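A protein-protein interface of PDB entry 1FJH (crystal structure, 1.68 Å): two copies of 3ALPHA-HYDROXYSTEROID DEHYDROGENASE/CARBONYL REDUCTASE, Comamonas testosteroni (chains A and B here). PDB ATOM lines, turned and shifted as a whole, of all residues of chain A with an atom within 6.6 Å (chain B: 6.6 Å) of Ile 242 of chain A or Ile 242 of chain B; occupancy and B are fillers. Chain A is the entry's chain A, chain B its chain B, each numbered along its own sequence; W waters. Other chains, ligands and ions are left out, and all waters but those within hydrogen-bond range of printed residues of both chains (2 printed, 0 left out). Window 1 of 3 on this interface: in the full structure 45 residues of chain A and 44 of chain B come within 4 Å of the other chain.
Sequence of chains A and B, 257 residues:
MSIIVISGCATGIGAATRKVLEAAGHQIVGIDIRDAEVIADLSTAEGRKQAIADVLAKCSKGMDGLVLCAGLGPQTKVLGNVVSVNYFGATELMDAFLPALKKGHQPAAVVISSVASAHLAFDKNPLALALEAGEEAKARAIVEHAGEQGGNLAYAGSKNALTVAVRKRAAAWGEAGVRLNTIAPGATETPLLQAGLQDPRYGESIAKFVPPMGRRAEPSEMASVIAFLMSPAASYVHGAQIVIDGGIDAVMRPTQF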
ATOM      1  N   ASN A 181      24.931 -10.488 -34.794  1.00  0.00           N
ATOM      2  CA  ASN A 181      24.728 -11.173 -33.520  1.00  0.00           C
ATOM      3  C   ASN A 181      24.379 -12.626 -33.772  1.00  0.00           C
ATOM      4  O   ASN A 181      24.072 -13.011 -34.895  1.00  0.00           O
ATOM      5  CB  ASN A 181      23.550 -10.551 -32.763  1.00  0.00           C
ATOM      6  CG  ASN A 181      23.800  -9.117 -32.353  1.00  0.00           C
ATOM      7  OD1 ASN A 181      24.599  -8.848 -31.458  1.00  0.00           O
ATOM      8  ND2 ASN A 181      23.104  -8.185 -33.000  1.00  0.00           N
ATOM      9  N   THR A 182      24.414 -13.432 -32.718  1.00  0.00           N
ATOM     10  CA  THR A 182      24.015 -14.826 -32.847  1.00  0.00           C
ATOM     11  C   THR A 182      22.891 -15.104 -31.865  1.00  0.00           C
ATOM     12  O   THR A 182      22.664 -14.339 -30.924  1.00  0.00           O
ATOM     13  CB  THR A 182      25.129 -15.822 -32.458  1.00  0.00           C
ATOM     14  OG1 THR A 182      25.396 -15.707 -31.054  1.00  0.00           O
ATOM     15  CG2 THR A 182      26.397 -15.564 -33.244  1.00  0.00           C
ATOM     16  N   ILE A 183      22.155 -16.180 -32.117  1.00  0.00           N
ATOM     17  CA  ILE A 183      21.163 -16.621 -31.150  1.00  0.00           C
ATOM     18  C   ILE A 183      21.671 -18.023 -30.836  1.00  0.00           C
ATOM     19  O   ILE A 183      22.309 -18.668 -31.680  1.00  0.00           O
ATOM     20  CB  ILE A 183      19.690 -16.678 -31.673  1.00  0.00           C
ATOM     21  CG1 ILE A 183      19.542 -17.627 -32.861  1.00  0.00           C
ATOM     22  CG2 ILE A 183      19.215 -15.273 -32.016  1.00  0.00           C
ATOM     23  CD1 ILE A 183      18.106 -18.094 -33.049  1.00  0.00           C
ATOM     24  N   ALA A 184      21.428 -18.479 -29.616  1.00  0.00           N
ATOM     25  CA  ALA A 184      21.878 -19.795 -29.212  1.00  0.00           C
ATOM     26  C   ALA A 184      20.702 -20.608 -28.702  1.00  0.00           C
ATOM     27  O   ALA A 184      20.392 -20.578 -27.513  1.00  0.00           O
ATOM     28  CB  ALA A 184      22.944 -19.666 -28.129  1.00  0.00           C
ATOM     29  N   PRO A 185      20.012 -21.325 -29.605  1.00  0.00           N
ATOM     30  CA  PRO A 185      18.863 -22.148 -29.213  1.00  0.00           C
ATOM     31  C   PRO A 185      19.320 -23.257 -28.265  1.00  0.00           C
ATOM     32  O   PRO A 185      20.462 -23.714 -28.340  1.00  0.00           O
ATOM     33  CB  PRO A 185      18.372 -22.725 -30.540  1.00  0.00           C
ATOM     34  CG  PRO A 185      18.787 -21.709 -31.545  1.00  0.00           C
ATOM     35  CD  PRO A 185      20.169 -21.309 -31.070  1.00  0.00           C
ATOM     36  N   VAL A 225      12.645 -13.837 -31.640  1.00  0.00           N
ATOM     37  CA  VAL A 225      13.850 -13.221 -31.086  1.00  0.00           C
ATOM     38  C   VAL A 225      14.708 -12.705 -32.242  1.00  0.00           C
ATOM     39  O   VAL A 225      15.314 -11.635 -32.158  1.00  0.00           O
ATOM     40  CB  VAL A 225      14.666 -14.228 -30.256  1.00  0.00           C
ATOM     41  CG1 VAL A 225      15.935 -13.562 -29.727  1.00  0.00           C
ATOM     42  CG2 VAL A 225      13.821 -14.751 -29.105  1.00  0.00           C
ATOM     43  N   PHE A 228      13.426  -9.516 -33.439  1.00  0.00           N
ATOM     44  CA  PHE A 228      13.845  -8.446 -32.541  1.00  0.00           C
ATOM     45  C   PHE A 228      15.268  -8.004 -32.878  1.00  0.00           C
ATOM     46  O   PHE A 228      15.537  -6.811 -33.024  1.00  0.00           O
ATOM     47  CB  PHE A 228      13.758  -8.913 -31.075  1.00  0.00           C
ATOM     48  CG  PHE A 228      14.745  -8.237 -30.154  1.00  0.00           C
ATOM     49  CD1 PHE A 228      15.836  -8.939 -29.660  1.00  0.00           C
ATOM     50  CD2 PHE A 228      14.611  -6.892 -29.822  1.00  0.00           C
ATOM     51  CE1 PHE A 228      16.786  -8.317 -28.849  1.00  0.00           C
ATOM     52  CE2 PHE A 228      15.557  -6.256 -29.010  1.00  0.00           C
ATOM     53  CZ  PHE A 228      16.645  -6.968 -28.524  1.00  0.00           C
ATOM     54  N   LEU A 229      16.178  -8.966 -33.008  1.00  0.00           N
ATOM     55  CA  LEU A 229      17.566  -8.649 -33.320  1.00  0.00           C
ATOM     56  C   LEU A 229      17.767  -7.986 -34.679  1.00  0.00           C
ATOM     57  O   LEU A 229      18.763  -7.309 -34.896  1.00  0.00           O
ATOM     58  CB  LEU A 229      18.421  -9.916 -33.240  1.00  0.00           C
ATOM     59  CG  LEU A 229      18.736 -10.417 -31.831  1.00  0.00           C
ATOM     60  CD1 LEU A 229      19.391 -11.793 -31.909  1.00  0.00           C
ATOM     61  CD2 LEU A 229      19.661  -9.426 -31.119  1.00  0.00           C
ATOM     62  N   VAL A 237      22.616  -3.521 -29.935  1.00  0.00           N
ATOM     63  CA  VAL A 237      23.001  -4.904 -29.670  1.00  0.00           C
ATOM     64  C   VAL A 237      23.859  -5.350 -30.849  1.00  0.00           C
ATOM     65  O   VAL A 237      23.383  -5.447 -31.985  1.00  0.00           O
ATOM     66  CB  VAL A 237      21.774  -5.828 -29.551  1.00  0.00           C
ATOM     67  CG1 VAL A 237      22.229  -7.252 -29.241  1.00  0.00           C
ATOM     68  CG2 VAL A 237      20.843  -5.329 -28.452  1.00  0.00           C
ATOM     69  N   ALA A 240      26.738  -9.736 -29.848  1.00  0.00           N
ATOM     70  CA  ALA A 240      26.221 -10.517 -28.732  1.00  0.00           C
ATOM     71  C   ALA A 240      25.660 -11.874 -29.125  1.00  0.00           C
ATOM     72  O   ALA A 240      25.317 -12.106 -30.286  1.00  0.00           O
ATOM     73  CB  ALA A 240      25.140  -9.715 -28.000  1.00  0.00           C
ATOM     74  N   GLN A 241      25.592 -12.770 -28.146  1.00  0.00           N
ATOM     75  CA  GLN A 241      25.011 -14.093 -28.347  1.00  0.00           C
ATOM     76  C   GLN A 241      23.819 -14.184 -27.401  1.00  0.00           C
ATOM     77  O   GLN A 241      23.975 -14.151 -26.182  1.00  0.00           O
ATOM     78  CB  GLN A 241      26.001 -15.219 -28.024  1.00  0.00           C
ATOM     79  CG  GLN A 241      25.305 -16.597 -27.988  1.00  0.00           C
ATOM     80  CD  GLN A 241      26.196 -17.736 -28.435  1.00  0.00           C
ATOM     81  OE1 GLN A 241      26.708 -18.517 -27.617  1.00  0.00           O
ATOM     82  NE2 GLN A 241      26.396 -17.833 -29.737  1.00  0.00           N
ATOM     83  N   ILE A 242      22.626 -14.293 -27.972  1.00  0.00           N
ATOM     84  CA  ILE A 242      21.414 -14.370 -27.171  1.00  0.00           C
ATOM     85  C   ILE A 242      20.962 -15.814 -27.001  1.00  0.00           C
ATOM     86  O   ILE A 242      20.580 -16.480 -27.966  1.00  0.00           O
ATOM     87  CB  ILE A 242      20.266 -13.553 -27.819  1.00  0.00           C
ATOM     88  CG1 ILE A 242      20.640 -12.064 -27.872  1.00  0.00           C
ATOM     89  CG2 ILE A 242      18.989 -13.723 -27.013  1.00  0.00           C
ATOM     90  CD1 ILE A 242      21.749 -11.719 -28.855  1.00  0.00           C
ATOM     91  N   VAL A 243      21.015 -16.293 -25.763  1.00  0.00           N
ATOM     92  CA  VAL A 243      20.612 -17.660 -25.457  1.00  0.00           C
ATOM     93  C   VAL A 243      19.090 -17.746 -25.348  1.00  0.00           C
ATOM     94  O   VAL A 243      18.470 -16.994 -24.599  1.00  0.00           O
ATOM     95  CB  VAL A 243      21.244 -18.132 -24.131  1.00  0.00           C
ATOM     96  CG1 VAL A 243      20.787 -19.548 -23.806  1.00  0.00           C
ATOM     97  CG2 VAL A 243      22.768 -18.067 -24.234  1.00  0.00           C
ATOM     98  N   ILE A 244      18.498 -18.671 -26.096  1.00  0.00           N
ATOM     99  CA  ILE A 244      17.049 -18.861 -26.094  1.00  0.00           C
ATOM    100  C   ILE A 244      16.833 -20.328 -25.751  1.00  0.00           C
ATOM    101  O   ILE A 244      16.726 -21.162 -26.647  1.00  0.00           O
ATOM    102  CB  ILE A 244      16.454 -18.588 -27.488  1.00  0.00           C
ATOM    103  CG1 ILE A 244      17.027 -17.285 -28.065  1.00  0.00           C
ATOM    104  CG2 ILE A 244      14.930 -18.495 -27.389  1.00  0.00           C
ATOM    105  CD1 ILE A 244      16.617 -17.040 -29.505  1.00  0.00           C
ATOM    106  N   ASN B 181      15.417 -12.314 -16.571  1.00  0.00           N
ATOM    107  CA  ASN B 181      16.616 -12.095 -17.379  1.00  0.00           C
ATOM    108  C   ASN B 181      17.305 -10.806 -16.960  1.00  0.00           C
ATOM    109  O   ASN B 181      16.753 -10.008 -16.207  1.00  0.00           O
ATOM    110  CB  ASN B 181      16.242 -11.959 -18.861  1.00  0.00           C
ATOM    111  CG  ASN B 181      15.604 -13.210 -19.425  1.00  0.00           C
ATOM    112  OD1 ASN B 181      16.276 -14.217 -19.634  1.00  0.00           O
ATOM    113  ND2 ASN B 181      14.298 -13.153 -19.677  1.00  0.00           N
ATOM    114  N   THR B 182      18.524 -10.609 -17.449  1.00  0.00           N
ATOM    115  CA  THR B 182      19.239  -9.376 -17.165  1.00  0.00           C
ATOM    116  C   THR B 182      19.670  -8.766 -18.489  1.00  0.00           C
ATOM    117  O   THR B 182      19.689  -9.439 -19.527  1.00  0.00           O
ATOM    118  CB  THR B 182      20.548  -9.597 -16.360  1.00  0.00           C
ATOM    119  OG1 THR B 182      21.496 -10.297 -17.180  1.00  0.00           O
ATOM    120  CG2 THR B 182      20.283 -10.389 -15.092  1.00  0.00           C
ATOM    121  N   ILE B 183      19.961  -7.474 -18.455  1.00  0.00           N
ATOM    122  CA  ILE B 183      20.525  -6.809 -19.617  1.00  0.00           C
ATOM    123  C   ILE B 183      21.846  -6.308 -19.045  1.00  0.00           C
ATOM    124  O   ILE B 183      21.972  -6.084 -17.830  1.00  0.00           O
ATOM    125  CB  ILE B 183      19.688  -5.609 -20.165  1.00  0.00           C
ATOM    126  CG1 ILE B 183      19.547  -4.496 -19.124  1.00  0.00           C
ATOM    127  CG2 ILE B 183      18.348  -6.113 -20.673  1.00  0.00           C
ATOM    128  CD1 ILE B 183      19.223  -3.149 -19.748  1.00  0.00           C
ATOM    129  N   ALA B 184      22.843  -6.163 -19.903  1.00  0.00           N
ATOM    130  CA  ALA B 184      24.142  -5.705 -19.450  1.00  0.00           C
ATOM    131  C   ALA B 184      24.646  -4.569 -20.321  1.00  0.00           C
ATOM    132  O   ALA B 184      25.310  -4.797 -21.333  1.00  0.00           O
ATOM    133  CB  ALA B 184      25.137  -6.871 -19.457  1.00  0.00           C
ATOM    134  N   PRO B 185      24.306  -3.322 -19.952  1.00  0.00           N
ATOM    135  CA  PRO B 185      24.734  -2.136 -20.700  1.00  0.00           C
ATOM    136  C   PRO B 185      26.261  -2.048 -20.708  1.00  0.00           C
ATOM    137  O   PRO B 185      26.918  -2.530 -19.786  1.00  0.00           O
ATOM    138  CB  PRO B 185      24.114  -0.985 -19.908  1.00  0.00           C
ATOM    139  CG  PRO B 185      22.891  -1.606 -19.300  1.00  0.00           C
ATOM    140  CD  PRO B 185      23.402  -2.950 -18.850  1.00  0.00           C
ATOM    141  N   VAL B 225      15.252  -2.973 -25.485  1.00  0.00           N
ATOM    142  CA  VAL B 225      15.634  -4.369 -25.299  1.00  0.00           C
ATOM    143  C   VAL B 225      14.863  -4.922 -24.098  1.00  0.00           C
ATOM    144  O   VAL B 225      14.421  -6.072 -24.107  1.00  0.00           O
ATOM    145  CB  VAL B 225      17.146  -4.516 -25.065  1.00  0.00           C
ATOM    146  CG1 VAL B 225      17.492  -5.977 -24.822  1.00  0.00           C
ATOM    147  CG2 VAL B 225      17.901  -3.984 -26.270  1.00  0.00           C
ATOM    148  N   PHE B 228      11.411  -5.755 -25.130  1.00  0.00           N
ATOM    149  CA  PHE B 228      11.407  -7.045 -25.821  1.00  0.00           C
ATOM    150  C   PHE B 228      11.413  -8.198 -24.807  1.00  0.00           C
ATOM    151  O   PHE B 228      10.628  -9.139 -24.916  1.00  0.00           O
ATOM    152  CB  PHE B 228      12.632  -7.149 -26.743  1.00  0.00           C
ATOM    153  CG  PHE B 228      13.107  -8.560 -26.969  1.00  0.00           C
ATOM    154  CD1 PHE B 228      14.290  -9.006 -26.385  1.00  0.00           C
ATOM    155  CD2 PHE B 228      12.367  -9.444 -27.745  1.00  0.00           C
ATOM    156  CE1 PHE B 228      14.726 -10.314 -26.571  1.00  0.00           C
ATOM    157  CE2 PHE B 228      12.795 -10.756 -27.937  1.00  0.00           C
ATOM    158  CZ  PHE B 228      13.973 -11.190 -27.352  1.00  0.00           C
ATOM    159  N   LEU B 229      12.295  -8.115 -23.816  1.00  0.00           N
ATOM    160  CA  LEU B 229      12.401  -9.156 -22.799  1.00  0.00           C
ATOM    161  C   LEU B 229      11.154  -9.310 -21.932  1.00  0.00           C
ATOM    162  O   LEU B 229      10.920 -10.365 -21.350  1.00  0.00           O
ATOM    163  CB  LEU B 229      13.621  -8.888 -21.914  1.00  0.00           C
ATOM    164  CG  LEU B 229      14.967  -9.224 -22.574  1.00  0.00           C
ATOM    165  CD1 LEU B 229      16.123  -8.676 -21.747  1.00  0.00           C
ATOM    166  CD2 LEU B 229      15.079 -10.740 -22.721  1.00  0.00           C
ATOM    167  N   VAL B 237      12.878 -16.973 -23.656  1.00  0.00           N
ATOM    168  CA  VAL B 237      14.116 -16.418 -23.117  1.00  0.00           C
ATOM    169  C   VAL B 237      13.987 -16.303 -21.600  1.00  0.00           C
ATOM    170  O   VAL B 237      13.151 -15.553 -21.093  1.00  0.00           O
ATOM    171  CB  VAL B 237      14.407 -15.010 -23.688  1.00  0.00           C
ATOM    172  CG1 VAL B 237      15.757 -14.507 -23.152  1.00  0.00           C
ATOM    173  CG2 VAL B 237      14.407 -15.054 -25.221  1.00  0.00           C
ATOM    174  N   ALA B 240      18.775 -15.535 -19.138  1.00  0.00           N
ATOM    175  CA  ALA B 240      19.838 -15.007 -19.994  1.00  0.00           C
ATOM    176  C   ALA B 240      20.291 -13.585 -19.663  1.00  0.00           C
ATOM    177  O   ALA B 240      19.572 -12.827 -19.021  1.00  0.00           O
ATOM    178  CB  ALA B 240      19.389 -15.068 -21.455  1.00  0.00           C
ATOM    179  N   GLN B 241      21.505 -13.249 -20.098  1.00  0.00           N
ATOM    180  CA  GLN B 241      22.064 -11.910 -19.920  1.00  0.00           C
ATOM    181  C   GLN B 241      22.295 -11.358 -21.322  1.00  0.00           C
ATOM    182  O   GLN B 241      23.140 -11.864 -22.058  1.00  0.00           O
ATOM    183  CB  GLN B 241      23.395 -11.931 -19.149  1.00  0.00           C
ATOM    184  CG  GLN B 241      24.140 -10.568 -19.194  1.00  0.00           C
ATOM    185  CD  GLN B 241      24.952 -10.259 -17.939  1.00  0.00           C
ATOM    186  OE1 GLN B 241      26.188 -10.326 -17.942  1.00  0.00           O
ATOM    187  NE2 GLN B 241      24.259  -9.911 -16.863  1.00  0.00           N
ATOM    188  N   ILE B 242      21.527 -10.337 -21.694  1.00  0.00           N
ATOM    189  CA  ILE B 242      21.655  -9.720 -23.009  1.00  0.00           C
ATOM    190  C   ILE B 242      22.588  -8.517 -22.934  1.00  0.00           C
ATOM    191  O   ILE B 242      22.281  -7.532 -22.265  1.00  0.00           O
ATOM    192  CB  ILE B 242      20.289  -9.247 -23.533  1.00  0.00           C
ATOM    193  CG1 ILE B 242      19.305 -10.419 -23.547  1.00  0.00           C
ATOM    194  CG2 ILE B 242      20.445  -8.647 -24.924  1.00  0.00           C
ATOM    195  CD1 ILE B 242      19.758 -11.601 -24.380  1.00  0.00           C
ATOM    196  N   VAL B 243      23.723  -8.612 -23.621  1.00  0.00           N
ATOM    197  CA  VAL B 243      24.716  -7.544 -23.639  1.00  0.00           C
ATOM    198  C   VAL B 243      24.312  -6.469 -24.649  1.00  0.00           C
ATOM    199  O   VAL B 243      24.053  -6.767 -25.811  1.00  0.00           O
ATOM    200  CB  VAL B 243      26.115  -8.087 -24.020  1.00  0.00           C
ATOM    201  CG1 VAL B 243      27.129  -6.949 -24.035  1.00  0.00           C
ATOM    202  CG2 VAL B 243      26.548  -9.172 -23.033  1.00  0.00           C
ATOM    203  N   ILE B 244      24.260  -5.220 -24.197  1.00  0.00           N
ATOM    204  CA  ILE B 244      23.880  -4.097 -25.057  1.00  0.00           C
ATOM    205  C   ILE B 244      25.033  -3.108 -24.940  1.00  0.00           C
ATOM    206  O   ILE B 244      25.027  -2.249 -24.061  1.00  0.00           O
ATOM    207  CB  ILE B 244      22.581  -3.437 -24.549  1.00  0.00           C
ATOM    208  CG1 ILE B 244      21.520  -4.515 -24.261  1.00  0.00           C
ATOM    209  CG2 ILE B 244      22.047  -2.464 -25.600  1.00  0.00           C
ATOM    210  CD1 ILE B 244      20.275  -3.977 -23.562  1.00  0.00           C
HETATM  211  O   HOH W   1      22.089 -14.502 -23.771  1.00  0.00           O
HETATM  212  O   HOH W   2      24.179 -11.204 -24.844  1.00  0.00           O
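Water W1 lies within hydrogen-bond range of the backbone NH of Val 243 of chain A (2.9 Å), the backbone carbonyl oxygen of Gln 241 of chain A (3.1 Å) and the backbone carbonyl oxygen of Gln 241 of chain B (3.3 Å).
Water W2 lies within hydrogen-bond range of the backbone NH of Val 243 of chain B, the backbone carbonyl oxygen of Gln 241 of chain B and the backbone carbonyl oxygen of Gln 241 of chain A.
Among the printed residues, merely in contact across the chains: Val 225 of chain A with Phe 228 of chain B (3.9 Å), Val 225 of chain A with Val 237 of chain B (3.9 Å), Phe 228 of chain A with Val 225 of chain B (3.9 Å), Phe 228 of chain A with Phe 228 of chain B (3.6 Å), Val 237 of chain A with Val 225 of chain B (3.9 Å), Val 237 of chain A with Val 243 of chain B (3.9 Å), Ala 240 of chain A with Val 243 of chain B (3.8 Å), Ile 242 of chain A with Ile 242 of chain B (3.5 Å), Val 243 of chain A with Val 237 of chain B (3.95 Å) and Val 243 of chain A with Ala 240 of chain B (3.8 Å).
Of the 14 printed residues of chain A, 6 touch a printed residue of chain B.
Hydrophobic or aromatic side chains of chain A within 4 Å of the printed part of chain B: Val 225, Phe 228, Val 237, Ala 240 and Ile 242.
Along chain A the printed residues that touch a printed residue of chain B span positions 225 to 243.
Among the printed residues, 10 pairs touch across the chains.
Among the printed residues, no Asp or Glu carboxylate lies within 4 Å of a Lys or Arg side-chain nitrogen of the other chain.
Of the printed residues of chain B, Ile 242 of chain A touches Ile 242 (3.5 Å).
Printed residues of chain A within 4 Å of Ile 242 of chain B: Ile 242.
Of the printed residues of chain A, Val 225 of chain B touches Phe 228 and Val 237.
Printed residues of chain A within 4 Å of Ala 240 of chain B: Val 243 (3.8 Å).
The nearest printed residue of chain B that does not touch Ala 240 of chain A is Ile 242 of chain B (5.7 Å).
Val 225 of chain A touches Phe 228 of chain B, and with the chains exchanged Phe 228 of chain A touches Val 225 of chain B.
Val 237 of chain A touches Val 243 of chain B, and with the chains exchanged Val 243 of chain A touches Val 237 of chain B.
Ala 240 of chain A touches Val 243 of chain B, and with the chains exchanged Val 243 of chain A touches Ala 240 of chain B.
Ile 242 of chain A touches its own counterpart, Ile 242 of chain B.
14 positions are printed for both chains.
ND2 of Asn 181 of chain A sits at hydrogen-bond distance from O of Val 237 of chain A.
N of Ala 240 of chain A is in hydrogen-bond range of OD1 of Asn 181 of chain A, at 2.8 Å.
The backbone NH (N) of Thr 182 of chain A is in hydrogen-bond range of the backbone carbonyl oxygen (O) of Ala 240 of chain A (2.9 Å).
O of Thr 182 of chain A lies within hydrogen-bond range of N of Ile 242 of chain A (3.0 Å).
The side-chain amide nitrogen (ND2) of Asn 181 of chain B is in hydrogen-bond range of the backbone carbonyl oxygen (O) of Val 237 of chain B (3.0 Å).
The backbone NH of Ile 242 of chain B lies within hydrogen-bond range of the backbone carbonyl oxygen of Thr 182 of chain B (3.0 Å).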
